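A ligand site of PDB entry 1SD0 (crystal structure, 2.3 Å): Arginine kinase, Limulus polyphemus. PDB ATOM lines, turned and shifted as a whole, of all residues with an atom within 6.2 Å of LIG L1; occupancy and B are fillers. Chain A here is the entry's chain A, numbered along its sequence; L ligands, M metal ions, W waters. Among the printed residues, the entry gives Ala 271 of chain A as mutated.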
ATOM      1  N   SER A  25      30.593   8.570  -0.029  1.00  0.00           N
ATOM      2  CA  SER A  25      30.162   9.962  -0.144  1.00  0.00           C
ATOM      3  C   SER A  25      31.313  10.916   0.118  1.00  0.00           C
ATOM      4  O   SER A  25      32.211  10.624   0.901  1.00  0.00           O
ATOM      5  CB  SER A  25      29.028  10.256   0.845  1.00  0.00           C
ATOM      6  OG  SER A  25      29.501  10.272   2.171  1.00  0.00           O
ATOM      7  N   SER A  56      21.959  14.954   6.558  1.00  0.00           N
ATOM      8  CA  SER A  56      21.489  14.201   5.400  1.00  0.00           C
ATOM      9  C   SER A  56      22.455  13.136   4.915  1.00  0.00           C
ATOM     10  O   SER A  56      22.043  12.037   4.533  1.00  0.00           O
ATOM     11  CB  SER A  56      21.170  15.155   4.243  1.00  0.00           C
ATOM     12  OG  SER A  56      20.784  14.415   3.093  1.00  0.00           O
ATOM     13  N   ASP A  62      24.425   6.256   1.460  1.00  0.00           N
ATOM     14  CA  ASP A  62      24.478   6.058   0.014  1.00  0.00           C
ATOM     15  C   ASP A  62      24.547   7.377  -0.757  1.00  0.00           C
ATOM     16  O   ASP A  62      24.512   7.378  -1.991  1.00  0.00           O
ATOM     17  CB  ASP A  62      23.277   5.228  -0.430  1.00  0.00           C
ATOM     18  CG  ASP A  62      21.956   5.916  -0.138  1.00  0.00           C
ATOM     19  OD1 ASP A  62      21.876   6.631   0.879  1.00  0.00           O
ATOM     20  OD2 ASP A  62      20.995   5.716  -0.916  1.00  0.00           O
ATOM     21  N   SER A  63      24.647   8.492  -0.042  1.00  0.00           N
ATOM     22  CA  SER A  63      24.750   9.812  -0.670  1.00  0.00           C
ATOM     23  C   SER A  63      26.069   9.901  -1.426  1.00  0.00           C
ATOM     24  O   SER A  63      27.025   9.184  -1.117  1.00  0.00           O
ATOM     25  CB  SER A  63      24.706  10.923   0.387  1.00  0.00           C
ATOM     26  OG  SER A  63      23.471  10.964   1.072  1.00  0.00           O
ATOM     27  N   GLY A  64      26.124  10.781  -2.418  1.00  0.00           N
ATOM     28  CA  GLY A  64      27.350  10.944  -3.173  1.00  0.00           C
ATOM     29  C   GLY A  64      28.114  12.131  -2.630  1.00  0.00           C
ATOM     30  O   GLY A  64      29.336  12.193  -2.678  1.00  0.00           O
ATOM     31  N   VAL A  65      27.361  13.081  -2.089  1.00  0.00           N
ATOM     32  CA  VAL A  65      27.919  14.295  -1.504  1.00  0.00           C
ATOM     33  C   VAL A  65      27.613  14.323  -0.011  1.00  0.00           C
ATOM     34  O   VAL A  65      28.520  14.392   0.813  1.00  0.00           O
ATOM     35  CB  VAL A  65      27.324  15.526  -2.184  1.00  0.00           C
ATOM     36  CG1 VAL A  65      27.853  16.795  -1.528  1.00  0.00           C
ATOM     37  CG2 VAL A  65      27.672  15.505  -3.661  1.00  0.00           C
ATOM     38  N   GLY A  66      26.331  14.308   0.329  1.00  0.00           N
ATOM     39  CA  GLY A  66      25.942  14.274   1.734  1.00  0.00           C
ATOM     40  C   GLY A  66      25.699  15.549   2.529  1.00  0.00           C
ATOM     41  O   GLY A  66      25.284  15.451   3.691  1.00  0.00           O
ATOM     42  N   ILE A  67      25.946  16.718   1.958  1.00  0.00           N
ATOM     43  CA  ILE A  67      25.725  17.952   2.726  1.00  0.00           C
ATOM     44  C   ILE A  67      24.893  19.004   2.003  1.00  0.00           C
ATOM     45  O   ILE A  67      24.640  18.905   0.800  1.00  0.00           O
ATOM     46  CB  ILE A  67      27.064  18.598   3.159  1.00  0.00           C
ATOM     47  CG1 ILE A  67      27.819  19.125   1.926  1.00  0.00           C
ATOM     48  CG2 ILE A  67      27.924  17.575   3.889  1.00  0.00           C
ATOM     49  CD1 ILE A  67      29.028  19.963   2.267  1.00  0.00           C
ATOM     50  N   TYR A  68      24.449  20.009   2.755  1.00  0.00           N
ATOM     51  CA  TYR A  68      23.657  21.112   2.243  1.00  0.00           C
ATOM     52  C   TYR A  68      23.995  22.358   3.075  1.00  0.00           C
ATOM     53  O   TYR A  68      24.598  22.248   4.155  1.00  0.00           O
ATOM     54  CB  TYR A  68      22.148  20.841   2.360  1.00  0.00           C
ATOM     55  CG  TYR A  68      21.625  19.679   1.523  1.00  0.00           C
ATOM     56  CD1 TYR A  68      21.685  18.367   2.000  1.00  0.00           C
ATOM     57  CD2 TYR A  68      21.063  19.903   0.267  1.00  0.00           C
ATOM     58  CE1 TYR A  68      21.189  17.302   1.248  1.00  0.00           C
ATOM     59  CE2 TYR A  68      20.560  18.837  -0.497  1.00  0.00           C
ATOM     60  CZ  TYR A  68      20.634  17.549  -0.005  1.00  0.00           C
ATOM     61  OH  TYR A  68      20.116  16.502  -0.745  1.00  0.00           O
ATOM     62  N   ARG A 126      18.772  23.519 -17.183  1.00  0.00           N
ATOM     63  CA  ARG A 126      18.188  24.249 -16.059  1.00  0.00           C
ATOM     64  C   ARG A 126      19.205  25.029 -15.254  1.00  0.00           C
ATOM     65  O   ARG A 126      20.411  24.767 -15.308  1.00  0.00           O
ATOM     66  CB  ARG A 126      17.420  23.298 -15.121  1.00  0.00           C
ATOM     67  CG  ARG A 126      18.232  22.187 -14.400  1.00  0.00           C
ATOM     68  CD  ARG A 126      19.130  22.686 -13.252  1.00  0.00           C
ATOM     69  NE  ARG A 126      19.552  21.594 -12.374  1.00  0.00           N
ATOM     70  CZ  ARG A 126      20.557  21.654 -11.508  1.00  0.00           C
ATOM     71  NH1 ARG A 126      20.859  20.595 -10.751  1.00  0.00           N
ATOM     72  NH2 ARG A 126      21.283  22.757 -11.386  1.00  0.00           N
ATOM     73  N   ASP A 192      11.969  13.479  -1.366  1.00  0.00           N
ATOM     74  CA  ASP A 192      13.287  12.926  -1.631  1.00  0.00           C
ATOM     75  C   ASP A 192      13.920  12.675  -0.251  1.00  0.00           C
ATOM     76  O   ASP A 192      13.958  13.581   0.591  1.00  0.00           O
ATOM     77  CB  ASP A 192      14.111  13.930  -2.440  1.00  0.00           C
ATOM     78  CG  ASP A 192      15.513  13.453  -2.716  1.00  0.00           C
ATOM     79  OD1 ASP A 192      16.281  13.289  -1.743  1.00  0.00           O
ATOM     80  OD2 ASP A 192      15.855  13.237  -3.901  1.00  0.00           O
ATOM     81  N   PHE A 194      17.045  12.327   0.725  1.00  0.00           N
ATOM     82  CA  PHE A 194      18.212  13.154   1.001  1.00  0.00           C
ATOM     83  C   PHE A 194      17.771  14.560   1.429  1.00  0.00           C
ATOM     84  O   PHE A 194      18.352  15.142   2.346  1.00  0.00           O
ATOM     85  CB  PHE A 194      19.109  13.221  -0.231  1.00  0.00           C
ATOM     86  CG  PHE A 194      19.444  11.882  -0.805  1.00  0.00           C
ATOM     87  CD1 PHE A 194      18.638  11.294  -1.773  1.00  0.00           C
ATOM     88  CD2 PHE A 194      20.548  11.164  -0.320  1.00  0.00           C
ATOM     89  CE1 PHE A 194      18.907  10.017  -2.248  1.00  0.00           C
ATOM     90  CE2 PHE A 194      20.818   9.880  -0.787  1.00  0.00           C
ATOM     91  CZ  PHE A 194      20.005   9.304  -1.759  1.00  0.00           C
ATOM     92  N   LEU A 195      16.742  15.087   0.773  1.00  0.00           N
ATOM     93  CA  LEU A 195      16.211  16.411   1.078  1.00  0.00           C
ATOM     94  C   LEU A 195      15.404  16.412   2.376  1.00  0.00           C
ATOM     95  O   LEU A 195      15.485  17.345   3.176  1.00  0.00           O
ATOM     96  CB  LEU A 195      15.325  16.918  -0.067  1.00  0.00           C
ATOM     97  CG  LEU A 195      15.969  17.405  -1.372  1.00  0.00           C
ATOM     98  CD1 LEU A 195      14.882  17.660  -2.404  1.00  0.00           C
ATOM     99  CD2 LEU A 195      16.754  18.683  -1.115  1.00  0.00           C
ATOM    100  N   GLU A 225      14.211  21.928  -4.168  1.00  0.00           N
ATOM    101  CA  GLU A 225      15.536  22.010  -3.574  1.00  0.00           C
ATOM    102  C   GLU A 225      15.987  23.466  -3.462  1.00  0.00           C
ATOM    103  O   GLU A 225      16.641  23.844  -2.486  1.00  0.00           O
ATOM    104  CB  GLU A 225      16.536  21.196  -4.385  1.00  0.00           C
ATOM    105  CG  GLU A 225      17.960  21.310  -3.867  1.00  0.00           C
ATOM    106  CD  GLU A 225      18.919  20.329  -4.523  1.00  0.00           C
ATOM    107  OE1 GLU A 225      20.131  20.623  -4.553  1.00  0.00           O
ATOM    108  OE2 GLU A 225      18.457  19.278  -4.993  1.00  0.00           O
ATOM    109  N   ARG A 229      13.940  27.052  -9.993  1.00  0.00           N
ATOM    110  CA  ARG A 229      14.672  26.233 -10.936  1.00  0.00           C
ATOM    111  C   ARG A 229      14.044  26.632 -12.270  1.00  0.00           C
ATOM    112  O   ARG A 229      12.875  26.343 -12.509  1.00  0.00           O
ATOM    113  CB  ARG A 229      14.474  24.733 -10.685  1.00  0.00           C
ATOM    114  CG  ARG A 229      15.304  24.162  -9.546  1.00  0.00           C
ATOM    115  CD  ARG A 229      16.788  24.323  -9.782  1.00  0.00           C
ATOM    116  NE  ARG A 229      17.561  23.737  -8.700  1.00  0.00           N
ATOM    117  CZ  ARG A 229      17.736  22.423  -8.533  1.00  0.00           C
ATOM    118  NH1 ARG A 229      17.195  21.579  -9.393  1.00  0.00           N
ATOM    119  NH2 ARG A 229      18.430  21.961  -7.502  1.00  0.00           N
ATOM    120  N   ALA A 271      22.436  23.619  -2.346  1.00  0.00           N
ATOM    121  CA  ALA A 271      23.449  22.575  -2.378  1.00  0.00           C
ATOM    122  C   ALA A 271      24.748  22.996  -3.075  1.00  0.00           C
ATOM    123  O   ALA A 271      24.740  23.804  -3.995  1.00  0.00           O
ATOM    124  CB  ALA A 271      22.877  21.340  -3.036  1.00  0.00           C
ATOM    125  N   PRO A 272      25.885  22.439  -2.618  1.00  0.00           N
ATOM    126  CA  PRO A 272      27.206  22.745  -3.175  1.00  0.00           C
ATOM    127  C   PRO A 272      27.440  22.307  -4.621  1.00  0.00           C
ATOM    128  O   PRO A 272      28.269  22.889  -5.321  1.00  0.00           O
ATOM    129  CB  PRO A 272      28.158  22.094  -2.183  1.00  0.00           C
ATOM    130  CG  PRO A 272      27.381  20.914  -1.677  1.00  0.00           C
ATOM    131  CD  PRO A 272      25.992  21.486  -1.495  1.00  0.00           C
ATOM    132  N   THR A 273      26.729  21.287  -5.082  1.00  0.00           N
ATOM    133  CA  THR A 273      26.920  20.857  -6.463  1.00  0.00           C
ATOM    134  C   THR A 273      26.254  21.808  -7.454  1.00  0.00           C
ATOM    135  O   THR A 273      26.565  21.793  -8.641  1.00  0.00           O
ATOM    136  CB  THR A 273      26.371  19.433  -6.708  1.00  0.00           C
ATOM    137  OG1 THR A 273      25.004  19.352  -6.267  1.00  0.00           O
ATOM    138  CG2 THR A 273      27.210  18.398  -5.973  1.00  0.00           C
ATOM    139  N   ASN A 274      25.347  22.655  -6.967  1.00  0.00           N
ATOM    140  CA  ASN A 274      24.638  23.574  -7.859  1.00  0.00           C
ATOM    141  C   ASN A 274      25.075  25.050  -7.830  1.00  0.00           C
ATOM    142  O   ASN A 274      24.393  25.917  -8.376  1.00  0.00           O
ATOM    143  CB  ASN A 274      23.132  23.477  -7.607  1.00  0.00           C
ATOM    144  CG  ASN A 274      22.560  22.137  -8.024  1.00  0.00           C
ATOM    145  OD1 ASN A 274      22.843  21.658  -9.128  1.00  0.00           O
ATOM    146  ND2 ASN A 274      21.752  21.534  -7.172  1.00  0.00           N
ATOM    147  N   ARG A 309      22.688   9.685 -14.829  1.00  0.00           N
ATOM    148  CA  ARG A 309      21.568   9.537 -13.898  1.00  0.00           C
ATOM    149  C   ARG A 309      20.496   8.638 -14.518  1.00  0.00           C
ATOM    150  O   ARG A 309      20.513   8.392 -15.720  1.00  0.00           O
ATOM    151  CB  ARG A 309      20.958  10.919 -13.568  1.00  0.00           C
ATOM    152  CG  ARG A 309      21.845  11.820 -12.721  1.00  0.00           C
ATOM    153  CD  ARG A 309      21.271  13.223 -12.567  1.00  0.00           C
ATOM    154  NE  ARG A 309      22.195  14.075 -11.812  1.00  0.00           N
ATOM    155  CZ  ARG A 309      21.828  15.104 -11.056  1.00  0.00           C
ATOM    156  NH1 ARG A 309      20.543  15.426 -10.927  1.00  0.00           N
ATOM    157  NH2 ARG A 309      22.741  15.795 -10.391  1.00  0.00           N
ATOM    158  N   GLU A 314      18.348  11.763 -10.676  1.00  0.00           N
ATOM    159  CA  GLU A 314      19.420  11.210  -9.847  1.00  0.00           C
ATOM    160  C   GLU A 314      18.857  10.158  -8.892  1.00  0.00           C
ATOM    161  O   GLU A 314      17.668  10.148  -8.596  1.00  0.00           O
ATOM    162  CB  GLU A 314      20.098  12.332  -9.048  1.00  0.00           C
ATOM    163  CG  GLU A 314      19.163  13.061  -8.090  1.00  0.00           C
ATOM    164  CD  GLU A 314      19.885  14.103  -7.271  1.00  0.00           C
ATOM    165  OE1 GLU A 314      21.114  14.224  -7.424  1.00  0.00           O
ATOM    166  OE2 GLU A 314      19.219  14.811  -6.481  1.00  0.00           O
ATOM    167  N   HIS A 315      19.731   9.275  -8.405  1.00  0.00           N
ATOM    168  CA  HIS A 315      19.353   8.201  -7.488  1.00  0.00           C
ATOM    169  C   HIS A 315      18.260   7.276  -8.029  1.00  0.00           C
ATOM    170  O   HIS A 315      17.501   6.698  -7.255  1.00  0.00           O
ATOM    171  CB  HIS A 315      18.891   8.781  -6.140  1.00  0.00           C
ATOM    172  CG  HIS A 315      19.907   9.676  -5.488  1.00  0.00           C
ATOM    173  ND1 HIS A 315      19.637  10.987  -5.169  1.00  0.00           N
ATOM    174  CD2 HIS A 315      21.181   9.441  -5.109  1.00  0.00           C
ATOM    175  CE1 HIS A 315      20.715  11.525  -4.614  1.00  0.00           C
ATOM    176  NE2 HIS A 315      21.662  10.611  -4.575  1.00  0.00           N
HETATM  177  N1  LIG L   1      22.307  14.927  -1.265  1.00  0.00           N
HETATM  178  C1  LIG L   1      22.363  13.974  -2.411  1.00  0.00           C
HETATM  179  C2  LIG L   1      23.669  13.180  -2.379  1.00  0.00           C
HETATM  180  O1  LIG L   1      24.677  13.704  -1.857  1.00  0.00           O
HETATM  181  C3  LIG L   1      22.260  14.709  -3.744  1.00  0.00           C
HETATM  182  C4  LIG L   1      23.421  15.666  -4.050  1.00  0.00           C
HETATM  183  C5  LIG L   1      23.466  16.045  -5.530  1.00  0.00           C
HETATM  184  N2  LIG L   1      22.155  16.441  -6.043  1.00  0.00           N
HETATM  185  C6  LIG L   1      21.486  17.524  -5.655  1.00  0.00           C
HETATM  186  N3  LIG L   1      22.006  18.348  -4.749  1.00  0.00           N
HETATM  187  N4  LIG L   1      20.283  17.772  -6.156  1.00  0.00           N
HETATM  188  O2  LIG L   1      23.668  12.041  -2.895  1.00  0.00           O
HETATM  189  P1  LG2 L   2      17.551  18.511 -11.621  1.00  0.00           P
HETATM  190  O1  LG2 L   2      17.166  18.629 -10.178  1.00  0.00           O
HETATM  191  O2  LG2 L   2      16.582  19.268 -12.463  1.00  0.00           O
HETATM  192  O3  LG2 L   2      18.939  18.958 -11.923  1.00  0.00           O
HETATM  193  P2  LG2 L   2      16.964  15.601 -11.358  1.00  0.00           P
HETATM  194  O4  LG2 L   2      16.442  15.956 -10.012  1.00  0.00           O
HETATM  195  O5  LG2 L   2      17.950  14.484 -11.460  1.00  0.00           O
HETATM  196  O6  LG2 L   2      17.577  16.937 -12.048  1.00  0.00           O
HETATM  197  O7  LG2 L   2      15.736  15.317 -12.378  1.00  0.00           O
HETATM  198  C1  LG2 L   2      14.522  16.100 -12.299  1.00  0.00           C
HETATM  199  C2  LG2 L   2      13.601  15.699 -13.455  1.00  0.00           C
HETATM  200  O8  LG2 L   2      14.259  16.110 -14.667  1.00  0.00           O
HETATM  201  C3  LG2 L   2      13.384  14.200 -13.667  1.00  0.00           C
HETATM  202  O9  LG2 L   2      12.046  14.013 -14.173  1.00  0.00           O
HETATM  203  C4  LG2 L   2      14.266  13.847 -14.859  1.00  0.00           C
HETATM  204  O10 LG2 L   2      13.714  12.720 -15.567  1.00  0.00           O
HETATM  205  C5  LG2 L   2      14.110  15.096 -15.685  1.00  0.00           C
HETATM  206  N1  LG2 L   2      15.096  15.297 -16.795  1.00  0.00           N
HETATM  207  C6  LG2 L   2      16.422  15.529 -16.699  1.00  0.00           C
HETATM  208  N2  LG2 L   2      16.971  15.707 -17.918  1.00  0.00           N
HETATM  209  C7  LG2 L   2      15.959  15.561 -18.768  1.00  0.00           C
HETATM  210  C8  LG2 L   2      16.103  15.466 -20.148  1.00  0.00           C
HETATM  211  N3  LG2 L   2      17.257  15.626 -20.822  1.00  0.00           N
HETATM  212  N4  LG2 L   2      14.959  15.130 -20.798  1.00  0.00           N
HETATM  213  C9  LG2 L   2      13.819  14.929 -20.138  1.00  0.00           C
HETATM  214  N5  LG2 L   2      13.712  15.022 -18.818  1.00  0.00           N
HETATM  215  C10 LG2 L   2      14.792  15.320 -18.098  1.00  0.00           C
HETATM  216 MG    MG M   1      16.522  17.597  -8.509  1.00  0.00          MG
HETATM  217  O   HOH W   1      22.471  13.457   1.190  1.00  0.00           O
HETATM  218  O   HOH W   2      24.264  16.789  -0.876  1.00  0.00           O
HETATM  219  O   HOH W   3      19.058  16.763  -3.163  1.00  0.00           O
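The backbone NH (N) of Gly 64 sits at hydrogen-bond distance from an oxygen (O2) of LIG L1, 2.8 Å away. O5 of LG2 L2 lies within salt-bridge range of NH1 of Arg 309 (2.8 Å). N4 of LIG L1 is in salt-bridge range of OE2 of Glu 225. An oxygen (O2) of LG2 L2 is in salt-bridge range of the guanidinium group (NH1) of Arg 229 (3.9 Å). An oxygen (O2) of LIG L1 is in hydrogen-bond range of a ring nitrogen (NE2) of His 315 (3.0 Å). An oxygen (O1) of LIG L1 sits at hydrogen-bond distance from the backbone NH of Val 65, at 2.8 Å. A nitrogen (N1) of LIG L1 is in hydrogen-bond range of the side-chain hydroxyl (OH) of Tyr 68. The backbone NH (N) of Gly 66 is in hydrogen-bond range of an oxygen (O1) of LIG L1 (2.8 Å). The guanidinium group (NE) of Arg 126 lies within salt-bridge range of an oxygen (O3) of LG2 L2 (2.7 Å). OE1 of Glu 314 is in salt-bridge range of N2 of LIG L1 (2.8 Å). An oxygen (O5) of LG2 L2 lies within hydrogen-bond range of the backbone NH of Glu 314 (2.9 Å).
Ser 63 touches LIG L1 (CA to O2, 3.3 Å). Phe 194 touches LIG L1 (CB to N1, 3.8 Å). CB of Ala 271 touches N3 of LIG L1 (3.6 Å). Thr 273 touches LIG L1. Hydrophobic or aromatic side chains that line LIG L1: Val 65, Tyr 68, Phe 194, Ala 271 and His 315. 11 residues have an atom within 4 Å of LIG L1: Ser 63, Gly 64, Val 65, Gly 66, Tyr 68, Phe 194, Glu 225, Ala 271, Thr 273, Glu 314 and His 315. The nearest printed residue that does not touch LIG L1 is Asn 274 (4.01 Å).
Water W2 lies within hydrogen-bond range of the backbone carbonyl oxygen (O) of Ile 67 (2.7 Å), a nitrogen (N1) of LIG L1 (2.7 Å) and the backbone NH (N) of Gly 66 (3.4 Å). Water W1 lies within hydrogen-bond range of the side-chain hydroxyl of Ser 63, the side-chain hydroxyl of Ser 56 and a nitrogen (N1) of LIG L1. Water W3 lies within hydrogen-bond range of the side-chain hydroxyl of Tyr 68 (2.7 Å), the side-chain carboxylate of Glu 225 (3.2 Å) and a nitrogen (N4) of LIG L1 (3.4 Å).
The side-chain carboxylate of Glu 225 lies within salt-bridge range of the guanidinium group of Arg 229, at 3.7 Å. The side-chain carboxylate of Asp 192 lies within hydrogen-bond range of the backbone NH of Phe 194 (2.8 Å). The side-chain carboxylate (OE1) of Glu 225 sits at hydrogen-bond distance from the side-chain amide nitrogen (ND2) of Asn 274 (3.2 Å). The side-chain hydroxyl (OG) of Ser 56 sits at hydrogen-bond distance from the backbone carbonyl oxygen (O) of Phe 194 (2.6 Å). NH2 of Arg 309 lies within salt-bridge range of OE1 of Glu 314, 3.7 Å away.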
